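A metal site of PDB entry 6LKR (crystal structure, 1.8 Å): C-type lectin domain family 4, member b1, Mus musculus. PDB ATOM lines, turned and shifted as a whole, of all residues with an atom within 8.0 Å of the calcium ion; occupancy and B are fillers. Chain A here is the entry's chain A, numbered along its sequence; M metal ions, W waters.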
ATOM      1  N   ARG A  74      18.340   3.937  10.870  1.00  0.00           N
ATOM      2  CA  ARG A  74      16.944   3.469  10.708  1.00  0.00           C
ATOM      3  C   ARG A  74      15.998   4.482  11.372  1.00  0.00           C
ATOM      4  O   ARG A  74      14.918   4.069  11.824  1.00  0.00           O
ATOM      5  CB  ARG A  74      16.769   2.057  11.293  1.00  0.00           C
ATOM      6  CG  ARG A  74      17.882   1.072  10.950  1.00  0.00           C
ATOM      7  CD  ARG A  74      17.984   0.674   9.482  1.00  0.00           C
ATOM      8  NE  ARG A  74      18.582   1.722   8.657  1.00  0.00           N
ATOM      9  CZ  ARG A  74      18.758   1.645   7.342  1.00  0.00           C
ATOM     10  NH1 ARG A  74      18.431   0.554   6.682  1.00  0.00           N
ATOM     11  NH2 ARG A  74      19.269   2.675   6.685  1.00  0.00           N
ATOM     12  N   TRP A  76      13.937   6.770  10.214  1.00  0.00           N
ATOM     13  CA  TRP A  76      13.173   7.145   9.002  1.00  0.00           C
ATOM     14  C   TRP A  76      12.361   8.413   9.285  1.00  0.00           C
ATOM     15  O   TRP A  76      11.699   8.490  10.332  1.00  0.00           O
ATOM     16  CB  TRP A  76      12.288   5.982   8.536  1.00  0.00           C
ATOM     17  CG  TRP A  76      13.079   4.733   8.309  1.00  0.00           C
ATOM     18  CD1 TRP A  76      13.093   3.602   9.087  1.00  0.00           C
ATOM     19  CD2 TRP A  76      14.031   4.495   7.258  1.00  0.00           C
ATOM     20  NE1 TRP A  76      13.980   2.687   8.574  1.00  0.00           N
ATOM     21  CE2 TRP A  76      14.563   3.208   7.452  1.00  0.00           C
ATOM     22  CE3 TRP A  76      14.464   5.245   6.154  1.00  0.00           C
ATOM     23  CZ2 TRP A  76      15.503   2.646   6.598  1.00  0.00           C
ATOM     24  CZ3 TRP A  76      15.404   4.690   5.307  1.00  0.00           C
ATOM     25  CH2 TRP A  76      15.910   3.414   5.521  1.00  0.00           C
ATOM     26  N   TRP A  91       7.399  -2.046   3.664  1.00  0.00           N
ATOM     27  CA  TRP A  91       8.740  -2.580   3.326  1.00  0.00           C
ATOM     28  C   TRP A  91       8.563  -3.957   2.676  1.00  0.00           C
ATOM     29  O   TRP A  91       7.769  -4.731   3.212  1.00  0.00           O
ATOM     30  CB  TRP A  91       9.622  -2.711   4.565  1.00  0.00           C
ATOM     31  CG  TRP A  91       9.905  -1.411   5.250  1.00  0.00           C
ATOM     32  CD1 TRP A  91       9.355  -0.958   6.406  1.00  0.00           C
ATOM     33  CD2 TRP A  91      10.845  -0.407   4.823  1.00  0.00           C
ATOM     34  NE1 TRP A  91       9.878   0.264   6.730  1.00  0.00           N
ATOM     35  CE2 TRP A  91      10.786   0.624   5.772  1.00  0.00           C
ATOM     36  CE3 TRP A  91      11.706  -0.290   3.728  1.00  0.00           C
ATOM     37  CZ2 TRP A  91      11.599   1.751   5.674  1.00  0.00           C
ATOM     38  CZ3 TRP A  91      12.496   0.837   3.621  1.00  0.00           C
ATOM     39  CH2 TRP A  91      12.433   1.839   4.585  1.00  0.00           C
ATOM     40  N   GLY A  94      12.708  -8.613   3.882  1.00  0.00           N
ATOM     41  CA  GLY A  94      14.181  -8.427   3.946  1.00  0.00           C
ATOM     42  C   GLY A  94      14.601  -6.970   3.824  1.00  0.00           C
ATOM     43  O   GLY A  94      15.805  -6.711   3.764  1.00  0.00           O
ATOM     44  N   GLU A  95      13.658  -6.019   3.785  1.00  0.00           N
ATOM     45  CA  GLU A  95      13.963  -4.566   3.751  1.00  0.00           C
ATOM     46  C   GLU A  95      13.414  -3.938   5.031  1.00  0.00           C
ATOM     47  O   GLU A  95      12.424  -4.416   5.594  1.00  0.00           O
ATOM     48  CB  GLU A  95      13.362  -3.900   2.515  1.00  0.00           C
ATOM     49  CG  GLU A  95      13.774  -4.538   1.206  1.00  0.00           C
ATOM     50  CD  GLU A  95      15.270  -4.541   0.904  1.00  0.00           C
ATOM     51  OE1 GLU A  95      16.006  -3.668   1.420  1.00  0.00           O
ATOM     52  OE2 GLU A  95      15.698  -5.403   0.125  1.00  0.00           O
ATOM     53  N   PRO A  96      14.008  -2.856   5.542  1.00  0.00           N
ATOM     54  CA  PRO A  96      15.285  -2.320   5.057  1.00  0.00           C
ATOM     55  C   PRO A  96      16.442  -3.307   5.275  1.00  0.00           C
ATOM     56  O   PRO A  96      16.315  -4.160   6.134  1.00  0.00           O
ATOM     57  CB  PRO A  96      15.527  -1.077   5.916  1.00  0.00           C
ATOM     58  CG  PRO A  96      14.196  -0.762   6.554  1.00  0.00           C
ATOM     59  CD  PRO A  96      13.448  -2.062   6.644  1.00  0.00           C
ATOM     60  N   SER A  97      17.534  -3.170   4.515  1.00  0.00           N
ATOM     61  CA  SER A  97      18.619  -4.170   4.430  1.00  0.00           C
ATOM     62  C   SER A  97      19.977  -3.606   4.896  1.00  0.00           C
ATOM     63  O   SER A  97      20.810  -4.418   5.304  1.00  0.00           O
ATOM     64  CB  SER A  97      18.700  -4.743   3.038  1.00  0.00           C
ATOM     65  OG  SER A  97      19.096  -3.759   2.102  1.00  0.00           O
ATOM     66  N   SER A  98      20.211  -2.294   4.854  1.00  0.00           N
ATOM     67  CA  SER A  98      21.569  -1.746   5.111  1.00  0.00           C
ATOM     68  C   SER A  98      21.539  -0.327   5.673  1.00  0.00           C
ATOM     69  O   SER A  98      20.914   0.557   5.056  1.00  0.00           O
ATOM     70  CB  SER A  98      22.400  -1.790   3.855  1.00  0.00           C
ATOM     71  OG  SER A  98      23.636  -1.117   4.073  1.00  0.00           O
ATOM     72  N   ASP A  99      22.303  -0.089   6.744  1.00  0.00           N
ATOM     73  CA  ASP A  99      22.439   1.265   7.337  1.00  0.00           C
ATOM     74  C   ASP A  99      23.159   2.206   6.362  1.00  0.00           C
ATOM     75  O   ASP A  99      23.061   3.406   6.598  1.00  0.00           O
ATOM     76  CB  ASP A  99      23.130   1.242   8.688  1.00  0.00           C
ATOM     77  CG  ASP A  99      22.774   2.464   9.526  1.00  0.00           C
ATOM     78  OD1 ASP A  99      21.581   2.811   9.551  1.00  0.00           O
ATOM     79  OD2 ASP A  99      23.696   3.060  10.126  1.00  0.00           O
ATOM     80  N   GLU A 101      22.258   2.484   3.257  1.00  0.00           N
ATOM     81  CA  GLU A 101      21.170   2.876   2.322  1.00  0.00           C
ATOM     82  C   GLU A 101      20.216   3.808   3.066  1.00  0.00           C
ATOM     83  O   GLU A 101      19.466   3.314   3.940  1.00  0.00           O
ATOM     84  CB  GLU A 101      20.482   1.631   1.786  1.00  0.00           C
ATOM     85  CG  GLU A 101      21.400   0.768   0.949  1.00  0.00           C
ATOM     86  CD  GLU A 101      20.755  -0.479   0.368  1.00  0.00           C
ATOM     87  OE1 GLU A 101      21.129  -0.841  -0.758  1.00  0.00           O
ATOM     88  OE2 GLU A 101      19.890  -1.077   1.035  1.00  0.00           O
ATOM     89  N   CYS A 103      18.006   6.275   1.608  1.00  0.00           N
ATOM     90  CA  CYS A 103      16.823   6.719   0.829  1.00  0.00           C
ATOM     91  C   CYS A 103      15.977   5.492   0.478  1.00  0.00           C
ATOM     92  O   CYS A 103      16.462   4.358   0.653  1.00  0.00           O
ATOM     93  CB  CYS A 103      17.226   7.505  -0.405  1.00  0.00           C
ATOM     94  SG  CYS A 103      17.940   9.116   0.019  1.00  0.00           S
ATOM     95  N   THR A 105      12.933   3.599  -2.072  1.00  0.00           N
ATOM     96  CA  THR A 105      12.181   3.458  -3.340  1.00  0.00           C
ATOM     97  C   THR A 105      11.017   2.505  -3.133  1.00  0.00           C
ATOM     98  O   THR A 105      11.049   1.705  -2.177  1.00  0.00           O
ATOM     99  CB  THR A 105      13.038   2.917  -4.488  1.00  0.00           C
ATOM    100  OG1 THR A 105      13.686   1.719  -4.043  1.00  0.00           O
ATOM    101  CG2 THR A 105      14.062   3.922  -4.954  1.00  0.00           C
ATOM    102  N   TYR A 107       8.916  -0.344  -5.443  1.00  0.00           N
ATOM    103  CA  TYR A 107       9.056  -1.128  -6.689  1.00  0.00           C
ATOM    104  C   TYR A 107       8.255  -2.412  -6.552  1.00  0.00           C
ATOM    105  O   TYR A 107       7.821  -2.785  -5.439  1.00  0.00           O
ATOM    106  CB  TYR A 107      10.535  -1.366  -7.025  1.00  0.00           C
ATOM    107  CG  TYR A 107      11.166  -2.563  -6.368  1.00  0.00           C
ATOM    108  CD1 TYR A 107      11.726  -2.488  -5.111  1.00  0.00           C
ATOM    109  CD2 TYR A 107      11.264  -3.767  -7.052  1.00  0.00           C
ATOM    110  CE1 TYR A 107      12.334  -3.586  -4.521  1.00  0.00           C
ATOM    111  CE2 TYR A 107      11.859  -4.873  -6.480  1.00  0.00           C
ATOM    112  CZ  TYR A 107      12.400  -4.792  -5.212  1.00  0.00           C
ATOM    113  OH  TYR A 107      12.981  -5.885  -4.652  1.00  0.00           O
ATOM    114  N   ARG A 109       7.713  -6.429  -6.974  1.00  0.00           N
ATOM    115  CA  ARG A 109       8.317  -7.790  -7.012  1.00  0.00           C
ATOM    116  C   ARG A 109       7.308  -8.740  -7.689  1.00  0.00           C
ATOM    117  O   ARG A 109       6.174  -8.817  -7.210  1.00  0.00           O
ATOM    118  CB  ARG A 109       8.671  -8.261  -5.600  1.00  0.00           C
ATOM    119  CG  ARG A 109       9.921  -7.609  -5.025  1.00  0.00           C
ATOM    120  CD  ARG A 109      10.377  -8.274  -3.744  1.00  0.00           C
ATOM    121  NE  ARG A 109      11.615  -7.714  -3.217  1.00  0.00           N
ATOM    122  CZ  ARG A 109      12.143  -8.002  -2.021  1.00  0.00           C
ATOM    123  NH1 ARG A 109      11.545  -8.851  -1.208  1.00  0.00           N
ATOM    124  NH2 ARG A 109      13.264  -7.412  -1.650  1.00  0.00           N
ATOM    125  N   TRP A 116       8.509  -1.267  -0.360  1.00  0.00           N
ATOM    126  CA  TRP A 116       9.614  -0.291  -0.201  1.00  0.00           C
ATOM    127  C   TRP A 116      10.948  -1.034  -0.062  1.00  0.00           C
ATOM    128  O   TRP A 116      10.980  -2.144   0.511  1.00  0.00           O
ATOM    129  CB  TRP A 116       9.406   0.594   1.010  1.00  0.00           C
ATOM    130  CG  TRP A 116       8.116   1.344   1.085  1.00  0.00           C
ATOM    131  CD1 TRP A 116       7.187   1.572   0.109  1.00  0.00           C
ATOM    132  CD2 TRP A 116       7.616   1.992   2.268  1.00  0.00           C
ATOM    133  NE1 TRP A 116       6.158   2.319   0.607  1.00  0.00           N
ATOM    134  CE2 TRP A 116       6.396   2.586   1.924  1.00  0.00           C
ATOM    135  CE3 TRP A 116       8.117   2.132   3.566  1.00  0.00           C
ATOM    136  CZ2 TRP A 116       5.643   3.304   2.856  1.00  0.00           C
ATOM    137  CZ3 TRP A 116       7.375   2.830   4.489  1.00  0.00           C
ATOM    138  CH2 TRP A 116       6.161   3.418   4.122  1.00  0.00           C
ATOM    139  N   ASN A 117      12.007  -0.368  -0.508  1.00  0.00           N
ATOM    140  CA  ASN A 117      13.401  -0.841  -0.460  1.00  0.00           C
ATOM    141  C   ASN A 117      14.269   0.344  -0.070  1.00  0.00           C
ATOM    142  O   ASN A 117      14.125   1.418  -0.706  1.00  0.00           O
ATOM    143  CB  ASN A 117      13.799  -1.430  -1.816  1.00  0.00           C
ATOM    144  CG  ASN A 117      15.254  -1.853  -1.895  1.00  0.00           C
ATOM    145  OD1 ASN A 117      15.835  -2.324  -0.920  1.00  0.00           O
ATOM    146  ND2 ASN A 117      15.839  -1.735  -3.084  1.00  0.00           N
ATOM    147  N   ASP A 118      15.134   0.188   0.928  1.00  0.00           N
ATOM    148  CA  ASP A 118      16.196   1.194   1.190  1.00  0.00           C
ATOM    149  C   ASP A 118      17.255   1.023   0.089  1.00  0.00           C
ATOM    150  O   ASP A 118      17.553  -0.122  -0.296  1.00  0.00           O
ATOM    151  CB  ASP A 118      16.734   1.121   2.624  1.00  0.00           C
ATOM    152  CG  ASP A 118      17.399  -0.194   2.999  1.00  0.00           C
ATOM    153  OD1 ASP A 118      17.082  -1.236   2.359  1.00  0.00           O
ATOM    154  OD2 ASP A 118      18.205  -0.169   3.937  1.00  0.00           O
ATOM    155  N   ILE A 119      17.701   2.124  -0.503  1.00  0.00           N
ATOM    156  CA  ILE A 119      18.769   2.116  -1.540  1.00  0.00           C
ATOM    157  C   ILE A 119      19.661   3.336  -1.313  1.00  0.00           C
ATOM    158  O   ILE A 119      19.272   4.222  -0.535  1.00  0.00           O
ATOM    159  CB  ILE A 119      18.225   2.124  -2.980  1.00  0.00           C
ATOM    160  CG1 ILE A 119      17.423   3.385  -3.298  1.00  0.00           C
ATOM    161  CG2 ILE A 119      17.436   0.852  -3.278  1.00  0.00           C
ATOM    162  CD1 ILE A 119      17.299   3.635  -4.788  1.00  0.00           C
ATOM    163  N   SER A 120      20.798   3.375  -1.996  1.00  0.00           N
ATOM    164  CA  SER A 120      21.722   4.538  -1.986  1.00  0.00           C
ATOM    165  C   SER A 120      20.985   5.760  -2.556  1.00  0.00           C
ATOM    166  O   SER A 120      20.347   5.645  -3.609  1.00  0.00           O
ATOM    167  CB  SER A 120      22.983   4.242  -2.761  1.00  0.00           C
ATOM    168  OG  SER A 120      23.542   5.450  -3.260  1.00  0.00           O
HETATM  169 CA    CA M   1      17.865  -2.335   0.516  1.00  0.00          CA
HETATM  170  O   HOH W   1      18.060  -4.625  -0.757  1.00  0.00           O
HETATM  171  O   HOH W   2      19.030  -2.612  -1.452  1.00  0.00           O
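The calcium ion is bound by OD1 of Asp 118 (2.3 Å), water W2 (2.3 Å), O of Asp 118 (2.4 Å), OE2 of Glu 101 (2.4 Å), OE1 of Glu 95 (2.5 Å), OG of Ser 97 (2.5 Å), OD1 of Asn 117 (2.5 Å) and water W1 (2.6 Å).
OD2 of Asp 118 is in hydrogen-bond range of N of Ser 98, at 3.1 Å. The guanidinium group (NH1) of Arg 74 lies within salt-bridge range of the side-chain carboxylate (OD2) of Asp 118, 2.8 Å away. NH2 of Arg 74 sits at hydrogen-bond distance from O of Glu 101 (2.8 Å). NH2 of Arg 109 lies within salt-bridge range of OE2 of Glu 95 (3.6 Å). N of Asn 117 is in hydrogen-bond range of O of Thr 105, at 2.8 Å.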
